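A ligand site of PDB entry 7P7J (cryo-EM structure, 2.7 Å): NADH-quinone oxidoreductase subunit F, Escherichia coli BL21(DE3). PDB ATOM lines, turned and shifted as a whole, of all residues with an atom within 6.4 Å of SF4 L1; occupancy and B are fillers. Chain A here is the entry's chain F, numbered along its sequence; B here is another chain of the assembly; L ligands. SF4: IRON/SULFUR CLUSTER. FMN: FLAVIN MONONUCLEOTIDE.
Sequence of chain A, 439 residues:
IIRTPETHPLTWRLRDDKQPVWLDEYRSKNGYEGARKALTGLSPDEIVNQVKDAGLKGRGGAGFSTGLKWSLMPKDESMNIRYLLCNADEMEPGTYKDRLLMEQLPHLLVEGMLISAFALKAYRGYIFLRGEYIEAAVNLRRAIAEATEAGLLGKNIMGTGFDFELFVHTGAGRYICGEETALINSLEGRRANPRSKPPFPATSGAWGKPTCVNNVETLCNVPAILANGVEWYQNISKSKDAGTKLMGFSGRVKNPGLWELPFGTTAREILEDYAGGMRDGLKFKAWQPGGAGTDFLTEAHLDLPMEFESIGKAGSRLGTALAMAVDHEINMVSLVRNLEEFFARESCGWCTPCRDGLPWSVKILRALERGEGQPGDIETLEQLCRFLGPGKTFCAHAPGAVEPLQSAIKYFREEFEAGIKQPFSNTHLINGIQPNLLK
The side-chain sulfur (SG) of Cys 354 binds an iron atom (FE2) of SF4 L1 (2.3 Å).
The backbone NH (N) of Cys 351 lies close to a sulfur (S3) of SF4 L1.
The side-chain sulfur of Cys 351 binds an iron atom (FE1) of SF4 L1 (2.3 Å).
SG of Cys 395 is bound to FE3 of SF4 L1.
S1 of SF4 L1 sits close to N of Cys 348, 3.5 Å away.
The side-chain sulfur of Cys 348 is bound to an iron atom (FE4) of SF4 L1, 2.3 Å away.
N of Trp 350 sits close to S3 of SF4 L1.
The side-chain hydroxyl (OG) of Ser 347 lies close to a sulfur (S3) of SF4 L1 (3.5 Å).
A sulfur (S3) of SF4 L1 sits close to the backbone NH (N) of Gly 349, at 3.6 Å.
CD1 of Ile 176 touches S1 of SF4 L1 (3.7 Å).
CG of Pro 194 touches S2 of SF4 L1, 3.6 Å away.
Thr 393 touches SF4 L1.
CB of Phe 394 touches S2 of SF4 L1, at 3.6 Å.
His 397 touches SF4 L1 (CD2 to S1, 3.7 Å).
CB of Ala 398 touches S4 of SF4 L1, 3.8 Å away.
Hydrophobic or aromatic side chains within 4 Å of SF4 L1: Ile 176, Pro 194, Phe 394, His 397 and Ala 398.
Of the 23 residues printed, 13 come within 4 Å of SF4 L1.
OG of Ser 347 lies close to SG of Cys 354 (3.1 Å).
The backbone NH of Phe 394 lies close to the side-chain sulfur of Cys 351 (3.3 Å).
SG of Cys 395 sits close to N of His 397 (3.2 Å).
The side-chain hydroxyl of Thr 393 sits at hydrogen-bond distance from the backbone carbonyl oxygen of Cys 395.
The backbone NH of Trp 350 lies close to the side-chain sulfur of Cys 348 (3.4 Å).
SG of Cys 348 lies close to ND2 of Asn 193 (3.3 Å).
O of Trp 350 is in hydrogen-bond range of NH1 of Arg 355, at 3.4 Å.
The side-chain hydroxyl (OG) of Ser 347 lies within hydrogen-bond range of the backbone NH (N) of Gly 349.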
ATOM      1  N   ILE A 176     -10.687  -8.617  22.736  1.00  0.00           N
ATOM      2  CA  ILE A 176     -10.737  -8.767  21.292  1.00  0.00           C
ATOM      3  C   ILE A 176     -10.909 -10.226  20.885  1.00  0.00           C
ATOM      4  O   ILE A 176     -11.278 -10.511  19.747  1.00  0.00           O
ATOM      5  CB  ILE A 176      -9.478  -8.128  20.669  1.00  0.00           C
ATOM      6  CG1 ILE A 176      -9.638  -7.893  19.167  1.00  0.00           C
ATOM      7  CG2 ILE A 176      -8.261  -8.981  20.934  1.00  0.00           C
ATOM      8  CD1 ILE A 176     -10.945  -7.243  18.782  1.00  0.00           C
ATOM      9  N   ALA A 192      -4.468 -12.568  19.119  1.00  0.00           N
ATOM     10  CA  ALA A 192      -5.847 -12.425  18.685  1.00  0.00           C
ATOM     11  C   ALA A 192      -6.043 -11.214  17.782  1.00  0.00           C
ATOM     12  O   ALA A 192      -6.880 -10.351  18.081  1.00  0.00           O
ATOM     13  CB  ALA A 192      -6.779 -12.350  19.892  1.00  0.00           C
ATOM     14  N   ASN A 193      -5.284 -11.120  16.710  1.00  0.00           N
ATOM     15  CA  ASN A 193      -5.602 -10.182  15.649  1.00  0.00           C
ATOM     16  C   ASN A 193      -6.733 -10.758  14.802  1.00  0.00           C
ATOM     17  O   ASN A 193      -6.657 -11.911  14.377  1.00  0.00           O
ATOM     18  CB  ASN A 193      -4.383  -9.921  14.765  1.00  0.00           C
ATOM     19  CG  ASN A 193      -3.214  -9.359  15.531  1.00  0.00           C
ATOM     20  OD1 ASN A 193      -2.166  -9.987  15.638  1.00  0.00           O
ATOM     21  ND2 ASN A 193      -3.382  -8.153  16.065  1.00  0.00           N
ATOM     22  N   PRO A 194      -7.798 -10.001  14.565  1.00  0.00           N
ATOM     23  CA  PRO A 194      -8.862 -10.485  13.689  1.00  0.00           C
ATOM     24  C   PRO A 194      -8.400 -10.582  12.248  1.00  0.00           C
ATOM     25  O   PRO A 194      -7.402  -9.972  11.844  1.00  0.00           O
ATOM     26  CB  PRO A 194      -9.967  -9.444  13.853  1.00  0.00           C
ATOM     27  CG  PRO A 194      -9.273  -8.232  14.325  1.00  0.00           C
ATOM     28  CD  PRO A 194      -8.118  -8.687  15.149  1.00  0.00           C
ATOM     29  N   GLU A 346      -8.125  -2.310  25.148  1.00  0.00           N
ATOM     30  CA  GLU A 346      -8.511  -3.603  24.593  1.00  0.00           C
ATOM     31  C   GLU A 346      -8.341  -3.648  23.083  1.00  0.00           C
ATOM     32  O   GLU A 346      -8.830  -4.584  22.447  1.00  0.00           O
ATOM     33  CB  GLU A 346      -9.935  -3.952  24.983  1.00  0.00           C
ATOM     34  CG  GLU A 346     -10.119  -4.174  26.464  1.00  0.00           C
ATOM     35  CD  GLU A 346      -9.145  -5.178  27.032  1.00  0.00           C
ATOM     36  OE1 GLU A 346      -9.070  -6.299  26.495  1.00  0.00           O
ATOM     37  OE2 GLU A 346      -8.451  -4.843  28.012  1.00  0.00           O
ATOM     38  N   SER A 347      -7.696  -2.646  22.501  1.00  0.00           N
ATOM     39  CA  SER A 347      -7.311  -2.705  21.108  1.00  0.00           C
ATOM     40  C   SER A 347      -6.296  -3.815  20.884  1.00  0.00           C
ATOM     41  O   SER A 347      -5.536  -4.164  21.797  1.00  0.00           O
ATOM     42  CB  SER A 347      -6.735  -1.363  20.659  1.00  0.00           C
ATOM     43  OG  SER A 347      -6.307  -1.398  19.316  1.00  0.00           O
ATOM     44  N   CYS A 348      -6.307  -4.395  19.694  1.00  0.00           N
ATOM     45  CA  CYS A 348      -5.322  -5.418  19.386  1.00  0.00           C
ATOM     46  C   CYS A 348      -4.080  -4.849  18.713  1.00  0.00           C
ATOM     47  O   CYS A 348      -3.088  -5.580  18.568  1.00  0.00           O
ATOM     48  CB  CYS A 348      -5.954  -6.487  18.504  1.00  0.00           C
ATOM     49  SG  CYS A 348      -5.887  -6.142  16.758  1.00  0.00           S
ATOM     50  N   GLY A 349      -4.096  -3.576  18.338  1.00  0.00           N
ATOM     51  CA  GLY A 349      -2.940  -2.921  17.779  1.00  0.00           C
ATOM     52  C   GLY A 349      -2.640  -3.216  16.333  1.00  0.00           C
ATOM     53  O   GLY A 349      -1.574  -2.838  15.842  1.00  0.00           O
ATOM     54  N   TRP A 350      -3.551  -3.894  15.627  1.00  0.00           N
ATOM     55  CA  TRP A 350      -3.281  -4.264  14.240  1.00  0.00           C
ATOM     56  C   TRP A 350      -3.358  -3.061  13.324  1.00  0.00           C
ATOM     57  O   TRP A 350      -2.489  -2.864  12.458  1.00  0.00           O
ATOM     58  CB  TRP A 350      -4.257  -5.337  13.772  1.00  0.00           C
ATOM     59  CG  TRP A 350      -4.085  -5.715  12.361  1.00  0.00           C
ATOM     60  CD1 TRP A 350      -4.931  -5.438  11.332  1.00  0.00           C
ATOM     61  CD2 TRP A 350      -2.991  -6.435  11.792  1.00  0.00           C
ATOM     62  NE1 TRP A 350      -4.434  -5.953  10.156  1.00  0.00           N
ATOM     63  CE2 TRP A 350      -3.244  -6.569  10.416  1.00  0.00           C
ATOM     64  CE3 TRP A 350      -1.823  -6.992  12.320  1.00  0.00           C
ATOM     65  CZ2 TRP A 350      -2.374  -7.229   9.562  1.00  0.00           C
ATOM     66  CZ3 TRP A 350      -0.963  -7.642  11.471  1.00  0.00           C
ATOM     67  CH2 TRP A 350      -1.244  -7.757  10.108  1.00  0.00           C
ATOM     68  N   CYS A 351      -4.394  -2.241  13.478  1.00  0.00           N
ATOM     69  CA  CYS A 351      -4.684  -1.225  12.482  1.00  0.00           C
ATOM     70  C   CYS A 351      -4.653   0.170  13.079  1.00  0.00           C
ATOM     71  O   CYS A 351      -4.989   0.380  14.249  1.00  0.00           O
ATOM     72  CB  CYS A 351      -6.016  -1.519  11.782  1.00  0.00           C
ATOM     73  SG  CYS A 351      -7.525  -1.036  12.590  1.00  0.00           S
ATOM     74  N   THR A 352      -4.221   1.117  12.244  1.00  0.00           N
ATOM     75  CA  THR A 352      -3.833   2.450  12.708  1.00  0.00           C
ATOM     76  C   THR A 352      -4.942   3.274  13.352  1.00  0.00           C
ATOM     77  O   THR A 352      -4.675   3.847  14.428  1.00  0.00           O
ATOM     78  CB  THR A 352      -3.201   3.221  11.537  1.00  0.00           C
ATOM     79  OG1 THR A 352      -2.049   2.509  11.068  1.00  0.00           O
ATOM     80  CG2 THR A 352      -2.775   4.616  11.968  1.00  0.00           C
ATOM     81  N   PRO A 353      -6.165   3.406  12.793  1.00  0.00           N
ATOM     82  CA  PRO A 353      -7.119   4.350  13.403  1.00  0.00           C
ATOM     83  C   PRO A 353      -7.526   4.008  14.822  1.00  0.00           C
ATOM     84  O   PRO A 353      -7.487   4.885  15.683  1.00  0.00           O
ATOM     85  CB  PRO A 353      -8.321   4.302  12.451  1.00  0.00           C
ATOM     86  CG  PRO A 353      -7.776   3.817  11.191  1.00  0.00           C
ATOM     87  CD  PRO A 353      -6.777   2.807  11.602  1.00  0.00           C
ATOM     88  N   CYS A 354      -7.835   2.743  15.106  1.00  0.00           N
ATOM     89  CA  CYS A 354      -8.143   2.334  16.473  1.00  0.00           C
ATOM     90  C   CYS A 354      -6.928   2.520  17.376  1.00  0.00           C
ATOM     91  O   CYS A 354      -6.997   3.269  18.361  1.00  0.00           O
ATOM     92  CB  CYS A 354      -8.639   0.890  16.457  1.00  0.00           C
ATOM     93  SG  CYS A 354      -8.713  -0.099  17.954  1.00  0.00           S
ATOM     94  N   ARG A 355      -5.787   1.961  16.970  1.00  0.00           N
ATOM     95  CA  ARG A 355      -4.580   1.892  17.805  1.00  0.00           C
ATOM     96  C   ARG A 355      -4.052   3.278  18.155  1.00  0.00           C
ATOM     97  O   ARG A 355      -3.586   3.497  19.286  1.00  0.00           O
ATOM     98  CB  ARG A 355      -3.510   1.070  17.083  1.00  0.00           C
ATOM     99  CG  ARG A 355      -2.092   1.253  17.622  1.00  0.00           C
ATOM    100  CD  ARG A 355      -1.033   0.601  16.760  1.00  0.00           C
ATOM    101  NE  ARG A 355      -0.668   1.439  15.629  1.00  0.00           N
ATOM    102  CZ  ARG A 355      -0.850   1.106  14.355  1.00  0.00           C
ATOM    103  NH1 ARG A 355      -1.358  -0.067  14.027  1.00  0.00           N
ATOM    104  NH2 ARG A 355      -0.505   1.957  13.402  1.00  0.00           N
ATOM    105  N   LEU A 358      -7.962   5.944  19.280  1.00  0.00           N
ATOM    106  CA  LEU A 358      -8.597   5.762  20.580  1.00  0.00           C
ATOM    107  C   LEU A 358      -7.780   6.332  21.736  1.00  0.00           C
ATOM    108  O   LEU A 358      -8.388   6.954  22.622  1.00  0.00           O
ATOM    109  CB  LEU A 358      -8.930   4.280  20.791  1.00  0.00           C
ATOM    110  CG  LEU A 358     -10.093   3.742  19.953  1.00  0.00           C
ATOM    111  CD1 LEU A 358     -10.460   2.347  20.388  1.00  0.00           C
ATOM    112  CD2 LEU A 358     -11.289   4.666  20.040  1.00  0.00           C
ATOM    113  N   THR A 393     -11.636   1.081   9.711  1.00  0.00           N
ATOM    114  CA  THR A 393     -10.788   0.236  10.532  1.00  0.00           C
ATOM    115  C   THR A 393     -10.864  -1.217  10.069  1.00  0.00           C
ATOM    116  O   THR A 393     -11.711  -1.590   9.263  1.00  0.00           O
ATOM    117  CB  THR A 393     -11.181   0.338  12.009  1.00  0.00           C
ATOM    118  OG1 THR A 393     -12.553  -0.021  12.166  1.00  0.00           O
ATOM    119  CG2 THR A 393     -10.981   1.752  12.496  1.00  0.00           C
ATOM    120  N   PHE A 394      -9.947  -2.032  10.597  1.00  0.00           N
ATOM    121  CA  PHE A 394      -9.824  -3.402  10.121  1.00  0.00           C
ATOM    122  C   PHE A 394     -10.942  -4.296  10.634  1.00  0.00           C
ATOM    123  O   PHE A 394     -11.426  -5.170   9.910  1.00  0.00           O
ATOM    124  CB  PHE A 394      -8.474  -3.963  10.525  1.00  0.00           C
ATOM    125  CG  PHE A 394      -8.106  -5.234   9.826  1.00  0.00           C
ATOM    126  CD1 PHE A 394      -7.678  -5.218   8.515  1.00  0.00           C
ATOM    127  CD2 PHE A 394      -8.207  -6.454  10.483  1.00  0.00           C
ATOM    128  CE1 PHE A 394      -7.353  -6.387   7.873  1.00  0.00           C
ATOM    129  CE2 PHE A 394      -7.868  -7.620   9.842  1.00  0.00           C
ATOM    130  CZ  PHE A 394      -7.446  -7.582   8.539  1.00  0.00           C
ATOM    131  N   CYS A 395     -11.376  -4.088  11.874  1.00  0.00           N
ATOM    132  CA  CYS A 395     -12.480  -4.870  12.434  1.00  0.00           C
ATOM    133  C   CYS A 395     -13.512  -3.939  13.060  1.00  0.00           C
ATOM    134  O   CYS A 395     -13.417  -2.723  12.924  1.00  0.00           O
ATOM    135  CB  CYS A 395     -11.962  -5.897  13.438  1.00  0.00           C
ATOM    136  SG  CYS A 395     -11.895  -5.339  15.147  1.00  0.00           S
ATOM    137  N   ALA A 396     -14.498  -4.511  13.742  1.00  0.00           N
ATOM    138  CA  ALA A 396     -15.634  -3.754  14.246  1.00  0.00           C
ATOM    139  C   ALA A 396     -15.456  -3.290  15.684  1.00  0.00           C
ATOM    140  O   ALA A 396     -16.417  -2.799  16.275  1.00  0.00           O
ATOM    141  CB  ALA A 396     -16.914  -4.584  14.129  1.00  0.00           C
ATOM    142  N   HIS A 397     -14.266  -3.438  16.251  1.00  0.00           N
ATOM    143  CA  HIS A 397     -14.034  -3.000  17.628  1.00  0.00           C
ATOM    144  C   HIS A 397     -14.071  -1.480  17.738  1.00  0.00           C
ATOM    145  O   HIS A 397     -14.624  -0.923  18.692  1.00  0.00           O
ATOM    146  CB  HIS A 397     -12.709  -3.547  18.143  1.00  0.00           C
ATOM    147  CG  HIS A 397     -12.201  -2.857  19.365  1.00  0.00           C
ATOM    148  ND1 HIS A 397     -12.654  -3.156  20.635  1.00  0.00           N
ATOM    149  CD2 HIS A 397     -11.253  -1.899  19.520  1.00  0.00           C
ATOM    150  CE1 HIS A 397     -12.019  -2.397  21.509  1.00  0.00           C
ATOM    151  NE2 HIS A 397     -11.169  -1.632  20.865  1.00  0.00           N
ATOM    152  N   ALA A 398     -13.485  -0.782  16.764  1.00  0.00           N
ATOM    153  CA  ALA A 398     -13.405   0.669  16.795  1.00  0.00           C
ATOM    154  C   ALA A 398     -14.712   1.396  16.456  1.00  0.00           C
ATOM    155  O   ALA A 398     -14.969   2.441  17.057  1.00  0.00           O
ATOM    156  CB  ALA A 398     -12.276   1.155  15.880  1.00  0.00           C
ATOM    157  N   PRO A 399     -15.551   0.931  15.506  1.00  0.00           N
ATOM    158  CA  PRO A 399     -16.896   1.518  15.419  1.00  0.00           C
ATOM    159  C   PRO A 399     -17.713   1.371  16.688  1.00  0.00           C
ATOM    160  O   PRO A 399     -18.396   2.323  17.108  1.00  0.00           O
ATOM    161  CB  PRO A 399     -17.529   0.762  14.251  1.00  0.00           C
ATOM    162  CG  PRO A 399     -16.413   0.411  13.392  1.00  0.00           C
ATOM    163  CD  PRO A 399     -15.275   0.097  14.318  1.00  0.00           C
ATOM    164  N   HIS B 175      -2.279  -3.140  22.575  1.00  0.00           N
ATOM    165  CA  HIS B 175      -3.065  -2.089  21.952  1.00  0.00           C
ATOM    166  C   HIS B 175      -2.320  -0.959  21.254  1.00  0.00           C
ATOM    167  O   HIS B 175      -2.544  -0.715  20.065  1.00  0.00           O
ATOM    168  CB  HIS B 175      -3.921  -1.484  23.056  1.00  0.00           C
ATOM    169  CG  HIS B 175      -3.235  -1.445  24.390  1.00  0.00           C
ATOM    170  ND1 HIS B 175      -2.447  -0.391  24.788  1.00  0.00           N
ATOM    171  CD2 HIS B 175      -3.199  -2.346  25.393  1.00  0.00           C
ATOM    172  CE1 HIS B 175      -1.955  -0.636  25.988  1.00  0.00           C
ATOM    173  NE2 HIS B 175      -2.391  -1.823  26.384  1.00  0.00           N
HETATM  174 FE1  SF4 L   1      -8.065  -2.502  14.315  1.00  0.00          FE
HETATM  175 FE2  SF4 L   1      -8.641  -2.129  16.832  1.00  0.00          FE
HETATM  176 FE3  SF4 L   1      -9.924  -4.135  15.479  1.00  0.00          FE
HETATM  177 FE4  SF4 L   1      -7.393  -4.461  16.154  1.00  0.00          FE
HETATM  178  S1  SF4 L   1      -9.136  -4.231  17.652  1.00  0.00           S
HETATM  179  S2  SF4 L   1      -8.246  -4.775  14.047  1.00  0.00           S
HETATM  180  S3  SF4 L   1      -6.508  -2.350  16.002  1.00  0.00           S
HETATM  181  S4  SF4 L   1     -10.130  -1.886  15.098  1.00  0.00           S
HETATM  182  N1  FMN L   2     -19.729 -12.261  20.389  1.00  0.00           N
HETATM  183  C2  FMN L   2     -19.940 -13.039  21.501  1.00  0.00           C
HETATM  184  O2  FMN L   2     -20.770 -13.939  21.455  1.00  0.00           O
HETATM  185  N3  FMN L   2     -19.223 -12.811  22.652  1.00  0.00           N
HETATM  186  C4  FMN L   2     -18.288 -11.802  22.697  1.00  0.00           C
HETATM  187  O4  FMN L   2     -17.648 -11.587  23.709  1.00  0.00           O
HETATM  188  C4A FMN L   2     -18.077 -11.018  21.569  1.00  0.00           C
HETATM  189  N5  FMN L   2     -17.149 -10.013  21.607  1.00  0.00           N
HETATM  190  C5A FMN L   2     -16.930  -9.235  20.489  1.00  0.00           C
HETATM  191  C6  FMN L   2     -15.989  -8.223  20.542  1.00  0.00           C
HETATM  192  C7  FMN L   2     -15.766  -7.433  19.428  1.00  0.00           C
HETATM  193  C7M FMN L   2     -14.743  -6.343  19.500  1.00  0.00           C
HETATM  194  C8  FMN L   2     -16.484  -7.655  18.262  1.00  0.00           C
HETATM  195  C8M FMN L   2     -16.248  -6.803  17.053  1.00  0.00           C
HETATM  196  C9  FMN L   2     -17.424  -8.667  18.209  1.00  0.00           C
HETATM  197  C9A FMN L   2     -17.659  -9.470  19.324  1.00  0.00           C
HETATM  198  N10 FMN L   2     -18.599 -10.488  19.288  1.00  0.00           N
HETATM  199  C10 FMN L   2     -18.801 -11.250  20.412  1.00  0.00           C
HETATM  200  C1' FMN L   2     -19.399 -10.779  18.056  1.00  0.00           C
HETATM  201  C2' FMN L   2     -18.676 -11.823  17.201  1.00  0.00           C
HETATM  202  O2' FMN L   2     -17.859 -11.182  16.254  1.00  0.00           O
HETATM  203  C3' FMN L   2     -19.643 -12.746  16.462  1.00  0.00           C
HETATM  204  O3' FMN L   2     -20.580 -11.980  15.739  1.00  0.00           O
HETATM  205  C4' FMN L   2     -20.369 -13.654  17.444  1.00  0.00           C
HETATM  206  O4' FMN L   2     -19.470 -14.112  18.429  1.00  0.00           O
HETATM  207  C5' FMN L   2     -21.010 -14.858  16.770  1.00  0.00           C
HETATM  208  O5' FMN L   2     -22.120 -14.426  16.016  1.00  0.00           O
HETATM  209  P   FMN L   2     -23.591 -14.943  16.413  1.00  0.00           P
HETATM  210  O1P FMN L   2     -24.254 -13.865  17.229  1.00  0.00           O
HETATM  211  O2P FMN L   2     -24.376 -15.228  15.152  1.00  0.00           O
HETATM  212  O3P FMN L   2     -23.493 -16.186  17.247  1.00  0.00           O
